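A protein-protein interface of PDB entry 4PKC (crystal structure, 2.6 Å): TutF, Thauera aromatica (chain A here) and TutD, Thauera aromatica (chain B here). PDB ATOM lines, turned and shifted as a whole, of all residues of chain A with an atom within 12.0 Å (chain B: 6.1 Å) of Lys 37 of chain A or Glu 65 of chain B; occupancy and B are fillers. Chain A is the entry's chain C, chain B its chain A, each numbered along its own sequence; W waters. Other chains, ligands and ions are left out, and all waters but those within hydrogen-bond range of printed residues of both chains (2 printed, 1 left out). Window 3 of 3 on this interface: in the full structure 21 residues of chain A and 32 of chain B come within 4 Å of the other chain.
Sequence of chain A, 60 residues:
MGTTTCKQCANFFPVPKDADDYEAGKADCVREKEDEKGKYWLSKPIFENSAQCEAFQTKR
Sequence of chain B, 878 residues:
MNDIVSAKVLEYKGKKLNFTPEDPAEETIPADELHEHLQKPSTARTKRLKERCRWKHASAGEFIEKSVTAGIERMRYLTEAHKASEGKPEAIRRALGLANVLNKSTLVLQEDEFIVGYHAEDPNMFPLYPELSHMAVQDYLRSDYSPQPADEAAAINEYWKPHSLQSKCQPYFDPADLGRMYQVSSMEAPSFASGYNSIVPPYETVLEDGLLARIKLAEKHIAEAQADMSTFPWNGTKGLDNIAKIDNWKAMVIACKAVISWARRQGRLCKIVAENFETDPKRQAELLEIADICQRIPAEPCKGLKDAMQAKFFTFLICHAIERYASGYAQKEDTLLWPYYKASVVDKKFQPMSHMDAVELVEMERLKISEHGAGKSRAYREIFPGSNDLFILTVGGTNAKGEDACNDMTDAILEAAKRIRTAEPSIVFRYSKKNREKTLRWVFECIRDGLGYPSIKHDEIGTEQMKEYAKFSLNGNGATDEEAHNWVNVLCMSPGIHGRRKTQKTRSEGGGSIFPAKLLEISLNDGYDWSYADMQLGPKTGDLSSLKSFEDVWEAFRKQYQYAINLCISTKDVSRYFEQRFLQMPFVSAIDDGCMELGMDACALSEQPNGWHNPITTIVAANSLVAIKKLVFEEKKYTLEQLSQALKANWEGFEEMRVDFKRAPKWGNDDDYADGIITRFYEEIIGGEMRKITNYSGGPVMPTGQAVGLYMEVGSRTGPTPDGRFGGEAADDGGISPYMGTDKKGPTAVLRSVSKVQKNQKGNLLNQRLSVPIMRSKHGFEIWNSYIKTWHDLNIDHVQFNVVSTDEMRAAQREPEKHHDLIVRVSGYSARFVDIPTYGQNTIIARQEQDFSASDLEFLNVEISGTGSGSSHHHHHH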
ATOM      1  N   GLU A  32      -0.594   5.555  -9.491  1.00  0.00           N
ATOM      2  CA  GLU A  32      -1.215   6.612  -8.705  1.00  0.00           C
ATOM      3  C   GLU A  32      -0.204   7.244  -7.756  1.00  0.00           C
ATOM      4  O   GLU A  32       0.509   6.542  -7.039  1.00  0.00           O
ATOM      5  CB  GLU A  32      -2.411   6.073  -7.920  1.00  0.00           C
ATOM      6  CG  GLU A  32      -3.064   7.101  -7.011  1.00  0.00           C
ATOM      7  CD  GLU A  32      -4.272   6.552  -6.279  1.00  0.00           C
ATOM      8  OE1 GLU A  32      -4.376   6.772  -5.053  1.00  0.00           O
ATOM      9  OE2 GLU A  32      -5.122   5.907  -6.930  1.00  0.00           O
ATOM     10  N   LYS A  33      -0.139   8.571  -7.763  1.00  0.00           N
ATOM     11  CA  LYS A  33       0.757   9.300  -6.873  1.00  0.00           C
ATOM     12  C   LYS A  33      -0.004  10.394  -6.134  1.00  0.00           C
ATOM     13  O   LYS A  33      -1.120  10.748  -6.515  1.00  0.00           O
ATOM     14  CB  LYS A  33       1.927   9.905  -7.654  1.00  0.00           C
ATOM     15  CG  LYS A  33       2.684   8.909  -8.520  1.00  0.00           C
ATOM     16  CD  LYS A  33       3.897   9.549  -9.176  1.00  0.00           C
ATOM     17  CE  LYS A  33       5.030   9.745  -8.184  1.00  0.00           C
ATOM     18  NZ  LYS A  33       5.571   8.442  -7.711  1.00  0.00           N
ATOM     19  N   GLU A  34       0.603  10.930  -5.080  1.00  0.00           N
ATOM     20  CA  GLU A  34      -0.033  11.979  -4.291  1.00  0.00           C
ATOM     21  C   GLU A  34       0.985  12.763  -3.471  1.00  0.00           C
ATOM     22  O   GLU A  34       1.678  12.201  -2.624  1.00  0.00           O
ATOM     23  CB  GLU A  34      -1.098  11.380  -3.369  1.00  0.00           C
ATOM     24  CG  GLU A  34      -1.856  12.409  -2.547  1.00  0.00           C
ATOM     25  CD  GLU A  34      -3.008  11.803  -1.771  1.00  0.00           C
ATOM     26  OE1 GLU A  34      -3.039  10.564  -1.617  1.00  0.00           O
ATOM     27  OE2 GLU A  34      -3.886  12.568  -1.318  1.00  0.00           O
ATOM     28  N   ASP A  35       1.069  14.064  -3.728  1.00  0.00           N
ATOM     29  CA  ASP A  35       1.955  14.934  -2.967  1.00  0.00           C
ATOM     30  C   ASP A  35       1.149  15.844  -2.051  1.00  0.00           C
ATOM     31  O   ASP A  35      -0.003  15.550  -1.731  1.00  0.00           O
ATOM     32  CB  ASP A  35       2.842  15.764  -3.900  1.00  0.00           C
ATOM     33  CG  ASP A  35       2.046  16.538  -4.934  1.00  0.00           C
ATOM     34  OD1 ASP A  35       0.836  16.766  -4.721  1.00  0.00           O
ATOM     35  OD2 ASP A  35       2.639  16.928  -5.962  1.00  0.00           O
ATOM     36  N   GLU A  36       1.754  16.952  -1.633  1.00  0.00           N
ATOM     37  CA  GLU A  36       1.108  17.864  -0.693  1.00  0.00           C
ATOM     38  C   GLU A  36      -0.080  18.589  -1.319  1.00  0.00           C
ATOM     39  O   GLU A  36      -0.962  19.069  -0.608  1.00  0.00           O
ATOM     40  CB  GLU A  36       2.116  18.885  -0.152  1.00  0.00           C
ATOM     41  CG  GLU A  36       2.622  19.894  -1.178  1.00  0.00           C
ATOM     42  CD  GLU A  36       3.639  19.302  -2.134  1.00  0.00           C
ATOM     43  OE1 GLU A  36       4.127  20.040  -3.017  1.00  0.00           O
ATOM     44  OE2 GLU A  36       3.951  18.100  -2.002  1.00  0.00           O
ATOM     45  N   LYS A  37      -0.103  18.663  -2.647  1.00  0.00           N
ATOM     46  CA  LYS A  37      -1.178  19.352  -3.358  1.00  0.00           C
ATOM     47  C   LYS A  37      -2.421  18.482  -3.498  1.00  0.00           C
ATOM     48  O   LYS A  37      -3.521  18.896  -3.139  1.00  0.00           O
ATOM     49  CB  LYS A  37      -0.704  19.800  -4.741  1.00  0.00           C
ATOM     50  CG  LYS A  37       0.312  20.925  -4.719  1.00  0.00           C
ATOM     51  CD  LYS A  37      -0.280  22.189  -4.130  1.00  0.00           C
ATOM     52  CE  LYS A  37       0.708  23.339  -4.197  1.00  0.00           C
ATOM     53  NZ  LYS A  37       0.137  24.600  -3.648  1.00  0.00           N
ATOM     54  N   GLY A  38      -2.245  17.275  -4.026  1.00  0.00           N
ATOM     55  CA  GLY A  38      -3.362  16.371  -4.222  1.00  0.00           C
ATOM     56  C   GLY A  38      -2.977  15.102  -4.954  1.00  0.00           C
ATOM     57  O   GLY A  38      -1.796  14.821  -5.159  1.00  0.00           O
ATOM     58  N   LYS A  39      -3.984  14.335  -5.359  1.00  0.00           N
ATOM     59  CA  LYS A  39      -3.764  13.055  -6.020  1.00  0.00           C
ATOM     60  C   LYS A  39      -3.807  13.190  -7.540  1.00  0.00           C
ATOM     61  O   LYS A  39      -4.577  13.985  -8.081  1.00  0.00           O
ATOM     62  CB  LYS A  39      -4.809  12.039  -5.552  1.00  0.00           C
ATOM     63  CG  LYS A  39      -4.641  10.645  -6.131  1.00  0.00           C
ATOM     64  CD  LYS A  39      -5.758   9.724  -5.672  1.00  0.00           C
ATOM     65  CE  LYS A  39      -5.803   9.622  -4.156  1.00  0.00           C
ATOM     66  NZ  LYS A  39      -6.920   8.750  -3.703  1.00  0.00           N
ATOM     67  N   TYR A  40      -2.972  12.414  -8.225  1.00  0.00           N
ATOM     68  CA  TYR A  40      -2.990  12.375  -9.683  1.00  0.00           C
ATOM     69  C   TYR A  40      -2.511  11.025 -10.208  1.00  0.00           C
ATOM     70  O   TYR A  40      -1.996  10.201  -9.453  1.00  0.00           O
ATOM     71  CB  TYR A  40      -2.136  13.506 -10.265  1.00  0.00           C
ATOM     72  CG  TYR A  40      -0.671  13.446  -9.896  1.00  0.00           C
ATOM     73  CD1 TYR A  40      -0.210  14.014  -8.716  1.00  0.00           C
ATOM     74  CD2 TYR A  40       0.254  12.837 -10.736  1.00  0.00           C
ATOM     75  CE1 TYR A  40       1.129  13.969  -8.377  1.00  0.00           C
ATOM     76  CE2 TYR A  40       1.596  12.786 -10.406  1.00  0.00           C
ATOM     77  CZ  TYR A  40       2.028  13.355  -9.225  1.00  0.00           C
ATOM     78  OH  TYR A  40       3.361  13.309  -8.890  1.00  0.00           O
ATOM     79  N   TRP A  41      -2.687  10.805 -11.507  1.00  0.00           N
ATOM     80  CA  TRP A  41      -2.314   9.540 -12.128  1.00  0.00           C
ATOM     81  C   TRP A  41      -1.404   9.750 -13.335  1.00  0.00           C
ATOM     82  O   TRP A  41      -1.540  10.733 -14.063  1.00  0.00           O
ATOM     83  CB  TRP A  41      -3.567   8.765 -12.542  1.00  0.00           C
ATOM     84  CG  TRP A  41      -4.425   8.366 -11.381  1.00  0.00           C
ATOM     85  CD1 TRP A  41      -4.389   7.182 -10.706  1.00  0.00           C
ATOM     86  CD2 TRP A  41      -5.446   9.153 -10.754  1.00  0.00           C
ATOM     87  NE1 TRP A  41      -5.324   7.180  -9.699  1.00  0.00           N
ATOM     88  CE2 TRP A  41      -5.987   8.379  -9.708  1.00  0.00           C
ATOM     89  CE3 TRP A  41      -5.956  10.435 -10.977  1.00  0.00           C
ATOM     90  CZ2 TRP A  41      -7.012   8.845  -8.887  1.00  0.00           C
ATOM     91  CZ3 TRP A  41      -6.973  10.897 -10.161  1.00  0.00           C
ATOM     92  CH2 TRP A  41      -7.490  10.104  -9.129  1.00  0.00           C
ATOM     93  N   GLU B  51      -7.369  25.939  -4.160  1.00  0.00           N
ATOM     94  CA  GLU B  51      -6.608  25.681  -2.947  1.00  0.00           C
ATOM     95  C   GLU B  51      -5.418  24.769  -3.219  1.00  0.00           C
ATOM     96  O   GLU B  51      -4.329  24.984  -2.688  1.00  0.00           O
ATOM     97  CB  GLU B  51      -7.509  25.066  -1.874  1.00  0.00           C
ATOM     98  CG  GLU B  51      -7.878  26.022  -0.750  1.00  0.00           C
ATOM     99  CD  GLU B  51      -6.719  26.291   0.192  1.00  0.00           C
ATOM    100  OE1 GLU B  51      -6.650  27.405   0.753  1.00  0.00           O
ATOM    101  OE2 GLU B  51      -5.878  25.385   0.376  1.00  0.00           O
ATOM    102  N   ARG B  52      -5.626  23.756  -4.053  1.00  0.00           N
ATOM    103  CA  ARG B  52      -4.578  22.787  -4.344  1.00  0.00           C
ATOM    104  C   ARG B  52      -3.946  23.045  -5.710  1.00  0.00           C
ATOM    105  O   ARG B  52      -3.280  22.174  -6.275  1.00  0.00           O
ATOM    106  CB  ARG B  52      -5.131  21.361  -4.275  1.00  0.00           C
ATOM    107  CG  ARG B  52      -6.007  20.958  -5.452  1.00  0.00           C
ATOM    108  CD  ARG B  52      -5.581  19.596  -5.985  1.00  0.00           C
ATOM    109  NE  ARG B  52      -6.223  19.268  -7.255  1.00  0.00           N
ATOM    110  CZ  ARG B  52      -5.758  19.638  -8.444  1.00  0.00           C
ATOM    111  NH1 ARG B  52      -6.407  19.293  -9.547  1.00  0.00           N
ATOM    112  NH2 ARG B  52      -4.647  20.357  -8.531  1.00  0.00           N
ATOM    113  N   CYS B  53      -4.152  24.251  -6.228  1.00  0.00           N
ATOM    114  CA  CYS B  53      -3.620  24.633  -7.532  1.00  0.00           C
ATOM    115  C   CYS B  53      -2.099  24.547  -7.568  1.00  0.00           C
ATOM    116  O   CYS B  53      -1.415  25.098  -6.706  1.00  0.00           O
ATOM    117  CB  CYS B  53      -4.067  26.048  -7.898  1.00  0.00           C
ATOM    118  SG  CYS B  53      -3.527  26.595  -9.536  1.00  0.00           S
ATOM    119  N   ARG B  54      -1.579  23.846  -8.569  1.00  0.00           N
ATOM    120  CA  ARG B  54      -0.139  23.719  -8.747  1.00  0.00           C
ATOM    121  C   ARG B  54       0.413  24.951  -9.453  1.00  0.00           C
ATOM    122  O   ARG B  54       0.706  24.916 -10.649  1.00  0.00           O
ATOM    123  CB  ARG B  54       0.195  22.451  -9.534  1.00  0.00           C
ATOM    124  CG  ARG B  54      -0.381  21.185  -8.924  1.00  0.00           C
ATOM    125  CD  ARG B  54       0.057  19.943  -9.681  1.00  0.00           C
ATOM    126  NE  ARG B  54      -0.491  18.727  -9.085  1.00  0.00           N
ATOM    127  CZ  ARG B  54       0.039  18.107  -8.035  1.00  0.00           C
ATOM    128  NH1 ARG B  54       1.133  18.588  -7.462  1.00  0.00           N
ATOM    129  NH2 ARG B  54      -0.526  17.007  -7.557  1.00  0.00           N
ATOM    130  N   TRP B  55       0.543  26.040  -8.700  1.00  0.00           N
ATOM    131  CA  TRP B  55       1.020  27.308  -9.237  1.00  0.00           C
ATOM    132  C   TRP B  55       2.407  27.168  -9.852  1.00  0.00           C
ATOM    133  O   TRP B  55       3.236  26.397  -9.367  1.00  0.00           O
ATOM    134  CB  TRP B  55       1.035  28.376  -8.143  1.00  0.00           C
ATOM    135  CG  TRP B  55      -0.256  28.481  -7.389  1.00  0.00           C
ATOM    136  CD1 TRP B  55      -0.525  27.971  -6.152  1.00  0.00           C
ATOM    137  CD2 TRP B  55      -1.455  29.132  -7.826  1.00  0.00           C
ATOM    138  NE1 TRP B  55      -1.817  28.268  -5.791  1.00  0.00           N
ATOM    139  CE2 TRP B  55      -2.409  28.980  -6.801  1.00  0.00           C
ATOM    140  CE3 TRP B  55      -1.814  29.831  -8.982  1.00  0.00           C
ATOM    141  CZ2 TRP B  55      -3.699  29.499  -6.898  1.00  0.00           C
ATOM    142  CZ3 TRP B  55      -3.093  30.346  -9.077  1.00  0.00           C
ATOM    143  CH2 TRP B  55      -4.021  30.177  -8.041  1.00  0.00           C
ATOM    144  N   LYS B  56       2.654  27.914 -10.923  1.00  0.00           N
ATOM    145  CA  LYS B  56       3.917  27.816 -11.641  1.00  0.00           C
ATOM    146  C   LYS B  56       4.624  29.163 -11.731  1.00  0.00           C
ATOM    147  O   LYS B  56       5.646  29.289 -12.406  1.00  0.00           O
ATOM    148  CB  LYS B  56       3.689  27.253 -13.043  1.00  0.00           C
ATOM    149  CG  LYS B  56       3.122  25.844 -13.065  1.00  0.00           C
ATOM    150  CD  LYS B  56       4.078  24.855 -12.421  1.00  0.00           C
ATOM    151  CE  LYS B  56       3.748  23.428 -12.824  1.00  0.00           C
ATOM    152  NZ  LYS B  56       2.315  23.096 -12.595  1.00  0.00           N
ATOM    153  N   HIS B  57       4.078  30.166 -11.051  1.00  0.00           N
ATOM    154  CA  HIS B  57       4.669  31.499 -11.075  1.00  0.00           C
ATOM    155  C   HIS B  57       5.946  31.539 -10.243  1.00  0.00           C
ATOM    156  O   HIS B  57       6.139  30.724  -9.341  1.00  0.00           O
ATOM    157  CB  HIS B  57       3.667  32.548 -10.582  1.00  0.00           C
ATOM    158  CG  HIS B  57       3.257  32.381  -9.153  1.00  0.00           C
ATOM    159  ND1 HIS B  57       2.701  31.219  -8.665  1.00  0.00           N
ATOM    160  CD2 HIS B  57       3.301  33.244  -8.108  1.00  0.00           C
ATOM    161  CE1 HIS B  57       2.432  31.366  -7.380  1.00  0.00           C
ATOM    162  NE2 HIS B  57       2.785  32.588  -7.019  1.00  0.00           N
ATOM    163  N   PHE B  63      11.009  29.694  -8.220  1.00  0.00           N
ATOM    164  CA  PHE B  63       9.602  29.315  -8.263  1.00  0.00           C
ATOM    165  C   PHE B  63       8.983  29.353  -6.871  1.00  0.00           C
ATOM    166  O   PHE B  63       9.633  29.011  -5.883  1.00  0.00           O
ATOM    167  CB  PHE B  63       9.433  27.922  -8.875  1.00  0.00           C
ATOM    168  CG  PHE B  63       9.824  27.847 -10.323  1.00  0.00           C
ATOM    169  CD1 PHE B  63       9.027  28.418 -11.300  1.00  0.00           C
ATOM    170  CD2 PHE B  63      10.984  27.195 -10.710  1.00  0.00           C
ATOM    171  CE1 PHE B  63       9.382  28.350 -12.633  1.00  0.00           C
ATOM    172  CE2 PHE B  63      11.344  27.123 -12.043  1.00  0.00           C
ATOM    173  CZ  PHE B  63      10.542  27.700 -13.004  1.00  0.00           C
ATOM    174  N   ILE B  64       7.724  29.772  -6.801  1.00  0.00           N
ATOM    175  CA  ILE B  64       7.022  29.888  -5.528  1.00  0.00           C
ATOM    176  C   ILE B  64       6.755  28.513  -4.927  1.00  0.00           C
ATOM    177  O   ILE B  64       6.989  28.291  -3.739  1.00  0.00           O
ATOM    178  CB  ILE B  64       5.695  30.649  -5.692  1.00  0.00           C
ATOM    179  CG1 ILE B  64       5.956  32.036  -6.281  1.00  0.00           C
ATOM    180  CG2 ILE B  64       4.974  30.764  -4.358  1.00  0.00           C
ATOM    181  CD1 ILE B  64       6.859  32.903  -5.431  1.00  0.00           C
ATOM    182  N   GLU B  65       6.272  27.589  -5.752  1.00  0.00           N
ATOM    183  CA  GLU B  65       6.059  26.215  -5.313  1.00  0.00           C
ATOM    184  C   GLU B  65       7.369  25.434  -5.372  1.00  0.00           C
ATOM    185  O   GLU B  65       8.174  25.625  -6.282  1.00  0.00           O
ATOM    186  CB  GLU B  65       4.987  25.533  -6.163  1.00  0.00           C
ATOM    187  CG  GLU B  65       3.601  26.143  -6.020  1.00  0.00           C
ATOM    188  CD  GLU B  65       3.048  26.015  -4.610  1.00  0.00           C
ATOM    189  OE1 GLU B  65       3.433  25.064  -3.897  1.00  0.00           O
ATOM    190  OE2 GLU B  65       2.227  26.870  -4.213  1.00  0.00           O
ATOM    191  N   LYS B  66       7.569  24.550  -4.401  1.00  0.00           N
ATOM    192  CA  LYS B  66       8.853  23.876  -4.222  1.00  0.00           C
ATOM    193  C   LYS B  66       9.095  22.730  -5.201  1.00  0.00           C
ATOM    194  O   LYS B  66      10.242  22.352  -5.445  1.00  0.00           O
ATOM    195  CB  LYS B  66       8.965  23.349  -2.789  1.00  0.00           C
ATOM    196  CG  LYS B  66       7.836  22.411  -2.389  1.00  0.00           C
ATOM    197  CD  LYS B  66       8.076  21.805  -1.018  1.00  0.00           C
ATOM    198  CE  LYS B  66       6.962  20.848  -0.643  1.00  0.00           C
ATOM    199  NZ  LYS B  66       7.252  20.163   0.643  1.00  0.00           N
ATOM    200  N   SER B  67       8.024  22.175  -5.758  1.00  0.00           N
ATOM    201  CA  SER B  67       8.145  20.986  -6.599  1.00  0.00           C
ATOM    202  C   SER B  67       8.359  21.322  -8.072  1.00  0.00           C
ATOM    203  O   SER B  67       8.537  20.428  -8.899  1.00  0.00           O
ATOM    204  CB  SER B  67       6.906  20.103  -6.446  1.00  0.00           C
ATOM    205  OG  SER B  67       6.824  19.566  -5.137  1.00  0.00           O
ATOM    206  N   VAL B  68       8.347  22.612  -8.393  1.00  0.00           N
ATOM    207  CA  VAL B  68       8.489  23.051  -9.775  1.00  0.00           C
ATOM    208  C   VAL B  68       9.913  22.847 -10.289  1.00  0.00           C
ATOM    209  O   VAL B  68      10.870  23.396  -9.742  1.00  0.00           O
ATOM    210  CB  VAL B  68       8.105  24.531  -9.935  1.00  0.00           C
ATOM    211  CG1 VAL B  68       8.196  24.945 -11.396  1.00  0.00           C
ATOM    212  CG2 VAL B  68       6.703  24.772  -9.395  1.00  0.00           C
ATOM    213  N   GLU B 111      -7.093  14.885  -9.812  1.00  0.00           N
ATOM    214  CA  GLU B 111      -8.415  14.842  -9.203  1.00  0.00           C
ATOM    215  C   GLU B 111      -9.164  16.150  -9.437  1.00  0.00           C
ATOM    216  O   GLU B 111      -8.547  17.193  -9.656  1.00  0.00           O
ATOM    217  CB  GLU B 111      -8.305  14.555  -7.703  1.00  0.00           C
ATOM    218  CG  GLU B 111      -7.392  15.512  -6.953  1.00  0.00           C
ATOM    219  CD  GLU B 111      -7.403  15.270  -5.457  1.00  0.00           C
ATOM    220  OE1 GLU B 111      -8.479  14.935  -4.919  1.00  0.00           O
ATOM    221  OE2 GLU B 111      -6.337  15.407  -4.820  1.00  0.00           O
ATOM    222  N   ASN B 124       4.055  18.863 -11.928  1.00  0.00           N
ATOM    223  CA  ASN B 124       4.841  19.934 -11.326  1.00  0.00           C
ATOM    224  C   ASN B 124       5.950  20.410 -12.253  1.00  0.00           C
ATOM    225  O   ASN B 124       6.736  21.288 -11.895  1.00  0.00           O
ATOM    226  CB  ASN B 124       5.442  19.475  -9.997  1.00  0.00           C
ATOM    227  CG  ASN B 124       4.386  19.133  -8.967  1.00  0.00           C
ATOM    228  OD1 ASN B 124       3.306  19.720  -8.952  1.00  0.00           O
ATOM    229  ND2 ASN B 124       4.694  18.177  -8.099  1.00  0.00           N
ATOM    230  N   TYR B 145      16.821  23.604 -11.143  1.00  0.00           N
ATOM    231  CA  TYR B 145      15.643  23.065 -11.810  1.00  0.00           C
ATOM    232  C   TYR B 145      16.012  22.306 -13.077  1.00  0.00           C
ATOM    233  O   TYR B 145      15.182  22.132 -13.966  1.00  0.00           O
ATOM    234  CB  TYR B 145      14.663  24.188 -12.142  1.00  0.00           C
ATOM    235  CG  TYR B 145      14.463  25.165 -11.007  1.00  0.00           C
ATOM    236  CD1 TYR B 145      13.726  24.812  -9.884  1.00  0.00           C
ATOM    237  CD2 TYR B 145      15.012  26.439 -11.057  1.00  0.00           C
ATOM    238  CE1 TYR B 145      13.541  25.701  -8.843  1.00  0.00           C
ATOM    239  CE2 TYR B 145      14.832  27.335 -10.022  1.00  0.00           C
ATOM    240  CZ  TYR B 145      14.096  26.961  -8.918  1.00  0.00           C
ATOM    241  OH  TYR B 145      13.914  27.850  -7.884  1.00  0.00           O
HETATM  242  O   HOH W   1      -3.498  16.599  -7.587  1.00  0.00           O
HETATM  243  O   HOH W   2      -6.174  17.625  -2.954  1.00  0.00           O
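The guanidinium group (NH2) of Arg 54 of chain B lies within hydrogen-bond range of the backbone carbonyl oxygen (O) of Gly 38 of chain A, 3.5 Å away.
The side-chain amide nitrogen (ND2) of Asn 124 of chain B is in hydrogen-bond range of the side-chain carboxylate (OD2) of Asp 35 of chain A.
The side-chain carboxylate of Glu 65 of chain B lies within salt-bridge range of the side-chain amino group of Lys 37 of chain A (3.1 Å).
The side-chain amino group of Lys 37 of chain A lies within hydrogen-bond range of the backbone carbonyl oxygen of Cys 53 of chain B (3.5 Å).
The guanidinium group of Arg 54 of chain B lies within salt-bridge range of the side-chain carboxylate of Asp 35 of chain A, 2.7 Å away.
The side-chain hydroxyl of Ser 67 of chain B is in hydrogen-bond range of the side-chain carboxylate of Glu 36 of chain A, 3.5 Å away.
N of Lys 39 of chain A is in hydrogen-bond range of OE2 of Glu 111 of chain B.
Water W1 lies within hydrogen-bond range of O of Lys 39 of chain A, NH2 of Arg 54 of chain B and O of Gly 38 of chain A.
Water W2 lies within hydrogen-bond range of OE2 of Glu 111 of chain B (2.9 Å) and O of Lys 37 of chain A (2.9 Å).
Glu 34 of chain A touches none of the printed residues of chain B.
Of the printed residues of chain B, Asp 35 of chain A touches Arg 54 and Asn 124.
Of the printed residues of chain B, Glu 36 of chain A touches Lys 66 (3.8 Å) and Ser 67 (3.5 Å).
Of the printed residues of chain B, Gly 38 of chain A touches Arg 54 (3.5 Å) and Glu 111 (3.2 Å).
Printed residues of chain B within 4 Å of Tyr 40 of chain A: Arg 54 (3.2 Å).
Of chain A, only Lys 37 (3.2 Å) comes within 4 Å of Arg 52 of chain B.
Cys 53 of chain B touches just one residue of chain A: Lys 37.
Of chain A, only Asp 35 (2.7 Å), Lys 37 (3.5 Å), Gly 38 (3.5 Å) and Tyr 40 (3.2 Å) come within 4 Å of Arg 54 of chain B.
His 57 of chain B touches none of the printed residues of chain A.
No residue of chain A comes within 4 Å of Phe 63 of chain B.
Ile 64 of chain B touches none of the printed residues of chain A.
Of the printed residues of chain A, Lys 66 of chain B touches Glu 36 (3.8 Å).
No residue of chain A comes within 4 Å of Val 68 of chain B.
Of the printed residues of chain A, Glu 111 of chain B touches Gly 38 and Lys 39.
N of Gly 38 of chain A sits at hydrogen-bond distance from OD1 of Asp 35 of chain A, at 3.2 Å.
OE1 of Glu 32 of chain A is in salt-bridge range of NZ of Lys 39 of chain A (3.5 Å).
NE1 of Trp 55 of chain B sits close to O of Cys 53 of chain B, at 3.3 Å.
NH1 of Arg 54 of chain B sits at hydrogen-bond distance from OD1 of Asn 124 of chain B (2.9 Å).
The guanidinium group (NH1) of Arg 52 of chain B is in hydrogen-bond range of the backbone carbonyl oxygen (O) of Glu 111 of chain B (3.0 Å).
The backbone NH (N) of Lys 33 of chain A sits at hydrogen-bond distance from the backbone carbonyl oxygen (O) of Tyr 40 of chain A (3.0 Å).
Among the printed residues, pairs that only touch across the chains: Glu 36 of chain A with Lys 66 of chain B (3.8 Å), Lys 37 of chain A with Arg 52 of chain B (3.2 Å), Lys 37 of chain A with Arg 54 of chain B (3.5 Å), Gly 38 of chain A with Glu 111 of chain B (3.2 Å) and Tyr 40 of chain A with Arg 54 of chain B (3.2 Å).
Of the 16 printed residues of chain B, 8 touch a printed residue of chain A.
Hydrophobic or aromatic side chains of chain A that line the printed part of chain B: Tyr 40.
Among the printed residues, Asp or Glu carboxylates within 4 Å of a Lys or Arg side-chain nitrogen of the other chain: Asp 35 of chain A with Arg 54 of chain B (2.7 Å) and Lys 37 of chain A with Glu 65 of chain B (3.1 Å).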
